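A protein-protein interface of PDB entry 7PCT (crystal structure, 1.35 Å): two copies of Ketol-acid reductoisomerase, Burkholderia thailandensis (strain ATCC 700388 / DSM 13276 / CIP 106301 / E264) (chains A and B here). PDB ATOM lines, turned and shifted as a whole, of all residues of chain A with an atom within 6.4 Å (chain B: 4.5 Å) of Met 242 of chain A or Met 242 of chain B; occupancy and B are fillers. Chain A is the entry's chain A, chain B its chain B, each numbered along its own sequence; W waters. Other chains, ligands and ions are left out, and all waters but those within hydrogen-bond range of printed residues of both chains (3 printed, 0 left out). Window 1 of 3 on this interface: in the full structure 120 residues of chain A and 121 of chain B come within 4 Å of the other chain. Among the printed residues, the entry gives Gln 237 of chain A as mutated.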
ATOM      1  N   TYR A 138      12.608   3.645   3.005  1.00  0.00           N
ATOM      2  CA  TYR A 138      13.426   3.518   4.237  1.00  0.00           C
ATOM      3  C   TYR A 138      13.587   4.890   4.899  1.00  0.00           C
ATOM      4  O   TYR A 138      13.098   5.902   4.397  1.00  0.00           O
ATOM      5  CB  TYR A 138      14.713   2.732   3.974  1.00  0.00           C
ATOM      6  CG  TYR A 138      15.544   3.110   2.776  1.00  0.00           C
ATOM      7  CD1 TYR A 138      16.620   3.970   2.899  1.00  0.00           C
ATOM      8  CD2 TYR A 138      15.336   2.503   1.543  1.00  0.00           C
ATOM      9  CE1 TYR A 138      17.435   4.268   1.819  1.00  0.00           C
ATOM     10  CE2 TYR A 138      16.149   2.780   0.455  1.00  0.00           C
ATOM     11  CZ  TYR A 138      17.206   3.663   0.595  1.00  0.00           C
ATOM     12  OH  TYR A 138      18.002   3.935  -0.480  1.00  0.00           O
ATOM     13  N   LEU A 203      12.629  -9.053  -6.494  1.00  0.00           N
ATOM     14  CA  LEU A 203      13.051  -7.924  -7.356  1.00  0.00           C
ATOM     15  C   LEU A 203      14.403  -7.364  -6.917  1.00  0.00           C
ATOM     16  O   LEU A 203      15.264  -7.216  -7.790  1.00  0.00           O
ATOM     17  CB  LEU A 203      11.984  -6.840  -7.386  1.00  0.00           C
ATOM     18  CG  LEU A 203      12.357  -5.674  -8.300  1.00  0.00           C
ATOM     19  CD1 LEU A 203      12.548  -6.109  -9.747  1.00  0.00           C
ATOM     20  CD2 LEU A 203      11.320  -4.584  -8.193  1.00  0.00           C
ATOM     21  N   LEU A 207      17.639  -7.450  -9.395  1.00  0.00           N
ATOM     22  CA  LEU A 207      18.253  -6.188  -9.893  1.00  0.00           C
ATOM     23  C   LEU A 207      19.755  -6.224  -9.604  1.00  0.00           C
ATOM     24  O   LEU A 207      20.546  -5.941 -10.517  1.00  0.00           O
ATOM     25  CB  LEU A 207      17.609  -4.968  -9.229  1.00  0.00           C
ATOM     26  CG  LEU A 207      16.197  -4.602  -9.683  1.00  0.00           C
ATOM     27  CD1 LEU A 207      15.660  -3.482  -8.812  1.00  0.00           C
ATOM     28  CD2 LEU A 207      16.160  -4.190 -11.146  1.00  0.00           C
ATOM     29  N   VAL A 211      22.915  -6.400 -12.384  1.00  0.00           N
ATOM     30  CA  VAL A 211      24.042  -5.434 -12.372  1.00  0.00           C
ATOM     31  C   VAL A 211      25.348  -6.234 -12.277  1.00  0.00           C
ATOM     32  O   VAL A 211      26.299  -5.976 -13.033  1.00  0.00           O
ATOM     33  CB  VAL A 211      23.850  -4.467 -11.194  1.00  0.00           C
ATOM     34  CG1 VAL A 211      25.139  -3.783 -10.787  1.00  0.00           C
ATOM     35  CG2 VAL A 211      22.746  -3.464 -11.493  1.00  0.00           C
ATOM     36  N   VAL A 232      27.703  -0.190 -14.730  1.00  0.00           N
ATOM     37  CA  VAL A 232      26.562  -1.063 -14.323  1.00  0.00           C
ATOM     38  C   VAL A 232      25.819  -0.446 -13.119  1.00  0.00           C
ATOM     39  O   VAL A 232      24.624  -0.724 -12.984  1.00  0.00           O
ATOM     40  CB  VAL A 232      26.960  -2.536 -14.120  1.00  0.00           C
ATOM     41  CG1 VAL A 232      27.472  -3.135 -15.423  1.00  0.00           C
ATOM     42  CG2 VAL A 232      27.963  -2.730 -12.992  1.00  0.00           C
ATOM     43  N   TYR A 233      26.448   0.417 -12.309  1.00  0.00           N
ATOM     44  CA  TYR A 233      25.731   1.208 -11.270  1.00  0.00           C
ATOM     45  C   TYR A 233      26.612   2.299 -10.649  1.00  0.00           C
ATOM     46  O   TYR A 233      26.046   3.243 -10.118  1.00  0.00           O
ATOM     47  CB  TYR A 233      25.169   0.310 -10.153  1.00  0.00           C
ATOM     48  CG  TYR A 233      26.200  -0.136  -9.152  1.00  0.00           C
ATOM     49  CD1 TYR A 233      27.016  -1.224  -9.416  1.00  0.00           C
ATOM     50  CD2 TYR A 233      26.394   0.554  -7.966  1.00  0.00           C
ATOM     51  CE1 TYR A 233      27.984  -1.639  -8.513  1.00  0.00           C
ATOM     52  CE2 TYR A 233      27.379   0.174  -7.068  1.00  0.00           C
ATOM     53  CZ  TYR A 233      28.174  -0.929  -7.342  1.00  0.00           C
ATOM     54  OH  TYR A 233      29.155  -1.318  -6.472  1.00  0.00           O
ATOM     55  N   GLY A 236      26.193   6.122 -10.840  1.00  0.00           N
ATOM     56  CA  GLY A 236      24.861   6.589 -10.427  1.00  0.00           C
ATOM     57  C   GLY A 236      23.900   6.698 -11.593  1.00  0.00           C
ATOM     58  O   GLY A 236      22.715   6.986 -11.355  1.00  0.00           O
ATOM     59  N   GLN A 237      24.349   6.451 -12.827  1.00  0.00           N
ATOM     60  CA  GLN A 237      23.453   6.641 -13.994  1.00  0.00           C
ATOM     61  C   GLN A 237      22.264   5.678 -13.895  1.00  0.00           C
ATOM     62  O   GLN A 237      21.127   6.118 -14.145  1.00  0.00           O
ATOM     63  CB  GLN A 237      24.202   6.467 -15.310  1.00  0.00           C
ATOM     64  CG  GLN A 237      23.351   6.786 -16.537  1.00  0.00           C
ATOM     65  CD  GLN A 237      24.054   6.410 -17.817  1.00  0.00           C
ATOM     66  OE1 GLN A 237      25.278   6.267 -17.852  1.00  0.00           O
ATOM     67  NE2 GLN A 237      23.277   6.254 -18.885  1.00  0.00           N
ATOM     68  N   MET A 238      22.497   4.402 -13.583  1.00  0.00           N
ATOM     69  CA  MET A 238      21.380   3.424 -13.558  1.00  0.00           C
ATOM     70  C   MET A 238      20.427   3.772 -12.403  1.00  0.00           C
ATOM     71  O   MET A 238      19.194   3.732 -12.622  1.00  0.00           O
ATOM     72  CB  MET A 238      21.892   1.986 -13.480  1.00  0.00           C
ATOM     73  CG  MET A 238      22.619   1.544 -14.762  1.00  0.00           C
ATOM     74  SD  MET A 238      21.603   1.477 -16.283  1.00  0.00           S
ATOM     75  CE  MET A 238      21.864   3.101 -16.987  1.00  0.00           C
ATOM     76  N   GLY A 239      20.946   4.154 -11.235  1.00  0.00           N
ATOM     77  CA  GLY A 239      20.100   4.614 -10.116  1.00  0.00           C
ATOM     78  C   GLY A 239      19.292   5.845 -10.502  1.00  0.00           C
ATOM     79  O   GLY A 239      18.089   5.893 -10.215  1.00  0.00           O
ATOM     80  N   LYS A 240      19.937   6.836 -11.118  1.00  0.00           N
ATOM     81  CA  LYS A 240      19.253   8.091 -11.526  1.00  0.00           C
ATOM     82  C   LYS A 240      18.132   7.740 -12.508  1.00  0.00           C
ATOM     83  O   LYS A 240      17.041   8.321 -12.394  1.00  0.00           O
ATOM     84  CB  LYS A 240      20.229   9.082 -12.161  1.00  0.00           C
ATOM     85  CG  LYS A 240      21.178   9.809 -11.217  1.00  0.00           C
ATOM     86  CD  LYS A 240      20.530  10.691 -10.156  1.00  0.00           C
ATOM     87  CE  LYS A 240      19.631  11.795 -10.662  1.00  0.00           C
ATOM     88  NZ  LYS A 240      19.244  12.684  -9.540  1.00  0.00           N
ATOM     89  N   MET A 241      18.385   6.833 -13.454  1.00  0.00           N
ATOM     90  CA  MET A 241      17.362   6.441 -14.460  1.00  0.00           C
ATOM     91  C   MET A 241      16.164   5.837 -13.708  1.00  0.00           C
ATOM     92  O   MET A 241      14.998   6.173 -14.020  1.00  0.00           O
ATOM     93  CB  MET A 241      17.938   5.455 -15.487  1.00  0.00           C
ATOM     94  CG  MET A 241      16.883   4.825 -16.408  1.00  0.00           C
ATOM     95  SD  MET A 241      17.520   3.474 -17.443  1.00  0.00           S
ATOM     96  CE  MET A 241      17.336   2.101 -16.303  1.00  0.00           C
ATOM     97  N   MET A 242      16.419   4.977 -12.722  1.00  0.00           N
ATOM     98  CA  MET A 242      15.325   4.297 -11.991  1.00  0.00           C
ATOM     99  C   MET A 242      14.577   5.275 -11.082  1.00  0.00           C
ATOM    100  O   MET A 242      13.347   5.137 -10.960  1.00  0.00           O
ATOM    101  CB  MET A 242      15.882   3.138 -11.173  1.00  0.00           C
ATOM    102  CG  MET A 242      16.151   1.958 -12.043  1.00  0.00           C
ATOM    103  SD  MET A 242      14.701   0.862 -12.142  1.00  0.00           S
ATOM    104  CE  MET A 242      14.848   0.087 -10.532  1.00  0.00           C
ATOM    105  N   LEU A 243      15.272   6.240 -10.483  1.00  0.00           N
ATOM    106  CA  LEU A 243      14.623   7.222  -9.583  1.00  0.00           C
ATOM    107  C   LEU A 243      13.860   8.264 -10.410  1.00  0.00           C
ATOM    108  O   LEU A 243      12.700   8.555 -10.079  1.00  0.00           O
ATOM    109  CB  LEU A 243      15.683   7.847  -8.679  1.00  0.00           C
ATOM    110  CG  LEU A 243      15.151   8.672  -7.515  1.00  0.00           C
ATOM    111  CD1 LEU A 243      14.142   7.891  -6.685  1.00  0.00           C
ATOM    112  CD2 LEU A 243      16.300   9.155  -6.641  1.00  0.00           C
ATOM    113  N   ASP A 244      14.444   8.757 -11.502  1.00  0.00           N
ATOM    114  CA  ASP A 244      13.717   9.674 -12.414  1.00  0.00           C
ATOM    115  C   ASP A 244      12.536   8.911 -13.029  1.00  0.00           C
ATOM    116  O   ASP A 244      11.453   9.509 -13.226  1.00  0.00           O
ATOM    117  CB  ASP A 244      14.634  10.242 -13.492  1.00  0.00           C
ATOM    118  CG  ASP A 244      15.636  11.277 -13.001  1.00  0.00           C
ATOM    119  OD1 ASP A 244      15.514  11.735 -11.832  1.00  0.00           O
ATOM    120  OD2 ASP A 244      16.516  11.631 -13.806  1.00  0.00           O
ATOM    121  N   GLY A 245      12.715   7.616 -13.306  1.00  0.00           N
ATOM    122  CA  GLY A 245      11.632   6.772 -13.834  1.00  0.00           C
ATOM    123  C   GLY A 245      10.434   6.752 -12.902  1.00  0.00           C
ATOM    124  O   GLY A 245       9.298   6.693 -13.393  1.00  0.00           O
ATOM    125  N   ALA A 246      10.649   6.782 -11.588  1.00  0.00           N
ATOM    126  CA  ALA A 246       9.523   6.815 -10.632  1.00  0.00           C
ATOM    127  C   ALA A 246       8.657   8.043 -10.930  1.00  0.00           C
ATOM    128  O   ALA A 246       7.426   7.960 -10.789  1.00  0.00           O
ATOM    129  CB  ALA A 246      10.003   6.821  -9.207  1.00  0.00           C
ATOM    130  N   ASP A 247       9.277   9.165 -11.296  1.00  0.00           N
ATOM    131  CA  ASP A 247       8.532  10.408 -11.614  1.00  0.00           C
ATOM    132  C   ASP A 247       7.802  10.220 -12.952  1.00  0.00           C
ATOM    133  O   ASP A 247       6.559  10.319 -12.975  1.00  0.00           O
ATOM    134  CB  ASP A 247       9.472  11.618 -11.600  1.00  0.00           C
ATOM    135  CG  ASP A 247       8.792  12.956 -11.836  1.00  0.00           C
ATOM    136  OD1 ASP A 247       7.563  13.036 -11.645  1.00  0.00           O
ATOM    137  OD2 ASP A 247       9.509  13.916 -12.217  1.00  0.00           O
ATOM    138  N   LEU A 250       9.773   4.705 -16.904  1.00  0.00           N
ATOM    139  CA  LEU A 250      11.140   4.236 -17.243  1.00  0.00           C
ATOM    140  C   LEU A 250      11.413   4.408 -18.742  1.00  0.00           C
ATOM    141  O   LEU A 250      12.515   4.845 -19.102  1.00  0.00           O
ATOM    142  CB  LEU A 250      11.299   2.794 -16.767  1.00  0.00           C
ATOM    143  CG  LEU A 250      11.346   2.659 -15.245  1.00  0.00           C
ATOM    144  CD1 LEU A 250      11.018   1.233 -14.824  1.00  0.00           C
ATOM    145  CD2 LEU A 250      12.710   3.082 -14.705  1.00  0.00           C
ATOM    146  N   VAL A 253      12.003   8.107 -19.456  1.00  0.00           N
ATOM    147  CA  VAL A 253      13.372   8.599 -19.128  1.00  0.00           C
ATOM    148  C   VAL A 253      14.282   8.387 -20.344  1.00  0.00           C
ATOM    149  O   VAL A 253      15.057   9.295 -20.672  1.00  0.00           O
ATOM    150  CB  VAL A 253      13.964   7.927 -17.879  1.00  0.00           C
ATOM    151  CG1 VAL A 253      15.459   8.195 -17.756  1.00  0.00           C
ATOM    152  CG2 VAL A 253      13.231   8.361 -16.627  1.00  0.00           C
ATOM    153  N   LEU B 207      17.113  -4.252 -16.900  1.00  0.00           N
ATOM    154  CA  LEU B 207      16.603  -3.702 -15.616  1.00  0.00           C
ATOM    155  C   LEU B 207      15.114  -3.375 -15.777  1.00  0.00           C
ATOM    156  O   LEU B 207      14.311  -3.762 -14.916  1.00  0.00           O
ATOM    157  CB  LEU B 207      17.383  -2.446 -15.225  1.00  0.00           C
ATOM    158  CG  LEU B 207      18.809  -2.664 -14.719  1.00  0.00           C
ATOM    159  CD1 LEU B 207      19.533  -1.336 -14.604  1.00  0.00           C
ATOM    160  CD2 LEU B 207      18.830  -3.395 -13.387  1.00  0.00           C
ATOM    161  N   VAL B 211      11.885  -5.152 -13.827  1.00  0.00           N
ATOM    162  CA  VAL B 211      10.862  -4.354 -13.100  1.00  0.00           C
ATOM    163  C   VAL B 211       9.484  -4.704 -13.669  1.00  0.00           C
ATOM    164  O   VAL B 211       8.545  -4.950 -12.896  1.00  0.00           O
ATOM    165  CB  VAL B 211      11.194  -2.861 -13.242  1.00  0.00           C
ATOM    166  CG1 VAL B 211       9.994  -1.984 -12.953  1.00  0.00           C
ATOM    167  CG2 VAL B 211      12.392  -2.494 -12.382  1.00  0.00           C
ATOM    168  N   MET B 238      13.234   1.412  -5.199  1.00  0.00           N
ATOM    169  CA  MET B 238      14.249   0.651  -5.970  1.00  0.00           C
ATOM    170  C   MET B 238      15.291   1.619  -6.554  1.00  0.00           C
ATOM    171  O   MET B 238      16.487   1.296  -6.471  1.00  0.00           O
ATOM    172  CB  MET B 238      13.599  -0.222  -7.045  1.00  0.00           C
ATOM    173  CG  MET B 238      12.786  -1.382  -6.445  1.00  0.00           C
ATOM    174  SD  MET B 238      13.738  -2.641  -5.507  1.00  0.00           S
ATOM    175  CE  MET B 238      13.604  -2.006  -3.839  1.00  0.00           C
ATOM    176  N   GLY B 239      14.887   2.785  -7.066  1.00  0.00           N
ATOM    177  CA  GLY B 239      15.836   3.807  -7.564  1.00  0.00           C
ATOM    178  C   GLY B 239      16.736   4.322  -6.453  1.00  0.00           C
ATOM    179  O   GLY B 239      17.950   4.451  -6.666  1.00  0.00           O
ATOM    180  N   LYS B 240      16.169   4.611  -5.283  1.00  0.00           N
ATOM    181  CA  LYS B 240      16.945   5.106  -4.119  1.00  0.00           C
ATOM    182  C   LYS B 240      17.980   4.050  -3.732  1.00  0.00           C
ATOM    183  O   LYS B 240      19.136   4.413  -3.458  1.00  0.00           O
ATOM    184  CB  LYS B 240      16.031   5.382  -2.924  1.00  0.00           C
ATOM    185  CG  LYS B 240      15.194   6.646  -3.021  1.00  0.00           C
ATOM    186  CD  LYS B 240      16.006   7.918  -3.188  1.00  0.00           C
ATOM    187  CE  LYS B 240      16.946   8.200  -2.038  1.00  0.00           C
ATOM    188  NZ  LYS B 240      17.611   9.516  -2.191  1.00  0.00           N
ATOM    189  N   MET B 241      17.581   2.781  -3.699  1.00  0.00           N
ATOM    190  CA  MET B 241      18.513   1.687  -3.328  1.00  0.00           C
ATOM    191  C   MET B 241      19.675   1.679  -4.338  1.00  0.00           C
ATOM    192  O   MET B 241      20.846   1.560  -3.922  1.00  0.00           O
ATOM    193  CB  MET B 241      17.799   0.328  -3.311  1.00  0.00           C
ATOM    194  CG  MET B 241      18.747  -0.877  -3.220  1.00  0.00           C
ATOM    195  SD  MET B 241      17.912  -2.468  -3.414  1.00  0.00           S
ATOM    196  CE  MET B 241      17.845  -2.555  -5.203  1.00  0.00           C
ATOM    197  N   MET B 242      19.393   1.812  -5.632  1.00  0.00           N
ATOM    198  CA  MET B 242      20.460   1.726  -6.664  1.00  0.00           C
ATOM    199  C   MET B 242      21.338   2.974  -6.644  1.00  0.00           C
ATOM    200  O   MET B 242      22.553   2.848  -6.893  1.00  0.00           O
ATOM    201  CB  MET B 242      19.854   1.537  -8.047  1.00  0.00           C
ATOM    202  CG  MET B 242      19.097   0.246  -8.129  1.00  0.00           C
ATOM    203  SD  MET B 242      18.612  -0.182  -9.786  1.00  0.00           S
ATOM    204  CE  MET B 242      20.163  -0.017 -10.671  1.00  0.00           C
ATOM    205  N   LEU B 243      20.767   4.130  -6.330  1.00  0.00           N
ATOM    206  CA  LEU B 243      21.545   5.389  -6.286  1.00  0.00           C
ATOM    207  C   LEU B 243      22.372   5.434  -4.995  1.00  0.00           C
ATOM    208  O   LEU B 243      23.570   5.729  -5.057  1.00  0.00           O
ATOM    209  CB  LEU B 243      20.570   6.555  -6.398  1.00  0.00           C
ATOM    210  CG  LEU B 243      21.214   7.898  -6.688  1.00  0.00           C
ATOM    211  CD1 LEU B 243      22.175   7.802  -7.862  1.00  0.00           C
ATOM    212  CD2 LEU B 243      20.141   8.943  -6.944  1.00  0.00           C
ATOM    213  N   ASP B 244      21.783   5.086  -3.854  1.00  0.00           N
ATOM    214  CA  ASP B 244      22.566   4.951  -2.599  1.00  0.00           C
ATOM    215  C   ASP B 244      23.625   3.854  -2.798  1.00  0.00           C
ATOM    216  O   ASP B 244      24.738   3.980  -2.256  1.00  0.00           O
ATOM    217  CB  ASP B 244      21.664   4.663  -1.399  1.00  0.00           C
ATOM    218  CG  ASP B 244      20.820   5.836  -0.913  1.00  0.00           C
ATOM    219  OD1 ASP B 244      21.010   6.977  -1.410  1.00  0.00           O
ATOM    220  OD2 ASP B 244      19.973   5.591  -0.031  1.00  0.00           O
ATOM    221  N   GLY B 245      23.289   2.781  -3.521  1.00  0.00           N
ATOM    222  CA  GLY B 245      24.259   1.708  -3.811  1.00  0.00           C
ATOM    223  C   GLY B 245      25.494   2.236  -4.523  1.00  0.00           C
ATOM    224  O   GLY B 245      26.602   1.737  -4.263  1.00  0.00           O
ATOM    225  N   ALA B 246      25.344   3.213  -5.415  1.00  0.00           N
ATOM    226  CA  ALA B 246      26.510   3.814  -6.107  1.00  0.00           C
ATOM    227  C   ALA B 246      27.481   4.379  -5.066  1.00  0.00           C
ATOM    228  O   ALA B 246      28.707   4.307  -5.274  1.00  0.00           O
ATOM    229  CB  ALA B 246      26.087   4.884  -7.080  1.00  0.00           C
ATOM    230  N   LEU B 250      25.821  -2.030  -3.217  1.00  0.00           N
ATOM    231  CA  LEU B 250      24.406  -2.479  -3.277  1.00  0.00           C
ATOM    232  C   LEU B 250      24.087  -3.413  -2.103  1.00  0.00           C
ATOM    233  O   LEU B 250      23.028  -3.266  -1.474  1.00  0.00           O
ATOM    234  CB  LEU B 250      24.150  -3.122  -4.638  1.00  0.00           C
ATOM    235  CG  LEU B 250      24.126  -2.113  -5.785  1.00  0.00           C
ATOM    236  CD1 LEU B 250      24.367  -2.794  -7.126  1.00  0.00           C
ATOM    237  CD2 LEU B 250      22.799  -1.355  -5.797  1.00  0.00           C
HETATM  238  O   HOH W   1      23.303   3.644  -9.635  1.00  0.00           O
HETATM  239  O   HOH W   2      27.811  -3.183  -4.894  1.00  0.00           O
HETATM  240  O   HOH W   3      12.536   3.863  -8.438  1.00  0.00           O
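Water W2 bridges the side-chain hydroxyl of Tyr 233 of chain A (2.8 Å) and the backbone NH of Leu 250 of chain B (2.8 Å).
Water W1 lies within hydrogen-bond range of O of Tyr 233 of chain A (2.8 Å), N of Gly 239 of chain A (2.9 Å) and O of Met 242 of chain B (3.0 Å).
Water W3 lies within hydrogen-bond range of N of Gly 239 of chain B (2.9 Å) and O of Met 242 of chain A (2.9 Å).
Met 238 of chain A touches Met 242 of chain B, and with the chains exchanged Met 242 of chain A touches Met 238 of chain B.
Gly 239 of chain A touches Met 242 of chain B, and with the chains exchanged Met 242 of chain A touches Gly 239 of chain B.
Lys 240 of chain A touches Leu 243 of chain B, and with the chains exchanged Leu 243 of chain A touches Lys 240 of chain B.
Met 242 of chain A touches its own counterpart, Met 242 of chain B.
12 positions are printed for both chains.
Of the 25 pairs that touch across the chains among the printed residues, 16 have their exchanged pair printed and touching as well.
Of the 12 printed residues of chain B, 12 touch a printed residue of chain A.
Printed residues of chain B that touch a printed residue of chain A: Leu 207, Val 211, Met 238, Gly 239, Lys 240, Met 241, Met 242, Leu 243, Asp 244, Gly 245, Ala 246 and Leu 250.
Hydrophobic or aromatic side chains of chain B within 4 Å of the printed part of chain A: Leu 207, Val 211, Met 238, Met 242, Leu 243, Ala 246 and Leu 250.
Along chain B the printed residues that touch a printed residue of chain A span positions 207 to 250.
Among the printed residues, 25 pairs touch across the chains.
Among the printed residues, no Asp or Glu carboxylate lies within 4 Å of a Lys or Arg side-chain nitrogen of the other chain.
Of the printed residues of chain B, Met 242 of chain A touches Met 238, Gly 239 and Met 242.
Met 242 of chain B touches three residues of chain A.
Of the printed residues of chain B, Tyr 138 of chain A touches Lys 240, Met 241 and Asp 244.
Of the printed residues of chain B, Leu 243 of chain A touches Gly 239, Lys 240 and Leu 243.
Printed residues of chain A within 4 Å of Met 238 of chain B: Leu 203 (3.9 Å), Leu 207 (3.9 Å) and Met 242 (3.7 Å).
Val 253 of chain A touches none of the printed residues of chain B.
The nearest printed residue of chain B that does not touch Met 242 of chain A is Val 211 of chain B (4.01 Å).
The nearest printed residue of chain A that does not touch Lys 240 of chain B is Gly 239 of chain A (5.4 Å).
The side-chain carboxylate (OD2) of Asp 244 of chain B is in hydrogen-bond range of the side-chain hydroxyl (OH) of Tyr 138 of chain A (2.6 Å).
OH of Tyr 138 of chain A is in hydrogen-bond range of N of Met 241 of chain B (3.4 Å).
The backbone carbonyl oxygen of Lys 240 of chain B lies within hydrogen-bond range of the side-chain hydroxyl of Tyr 138 of chain A, at 3.2 Å.
Among the printed residues, pairs that only touch across the chains: Tyr 233 of chain A with Gly 245 of chain B (3.3 Å), Tyr 233 of chain A with Ala 246 of chain B (3.5 Å), Leu 207 of chain A with Leu 207 of chain B (3.6 Å), Gly 236 of chain A with Leu 243 of chain B (3.6 Å), Met 242 of chain A with Gly 239 of chain B (3.7 Å), Lys 240 of chain A with Leu 243 of chain B (3.7 Å), Leu 243 of chain A with Lys 240 of chain B (3.7 Å), Gly 239 of chain A with Met 242 of chain B (3.7 Å), Met 242 of chain A with Met 238 of chain B (3.7 Å), Tyr 233 of chain A with Leu 250 of chain B (3.8 Å), Gly 239 of chain A with Gly 239 of chain B (3.8 Å), Leu 243 of chain A with Gly 239 of chain B (3.8 Å), Met 242 of chain A with Met 242 of chain B (3.8 Å), Leu 243 of chain A with Leu 243 of chain B (3.9 Å), Met 238 of chain A with Met 242 of chain B (3.9 Å), Leu 250 of chain A with Val 211 of chain B (3.9 Å), Val 211 of chain A with Leu 250 of chain B (3.9 Å), Gly 239 of chain A with Leu 243 of chain B (3.9 Å), Met 238 of chain A with Leu 207 of chain B (3.9 Å), Leu 207 of chain A with Met 238 of chain B (3.9 Å), Leu 203 of chain A with Met 238 of chain B (3.9 Å) and Gly 236 of chain A with Ala 246 of chain B (3.95 Å).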
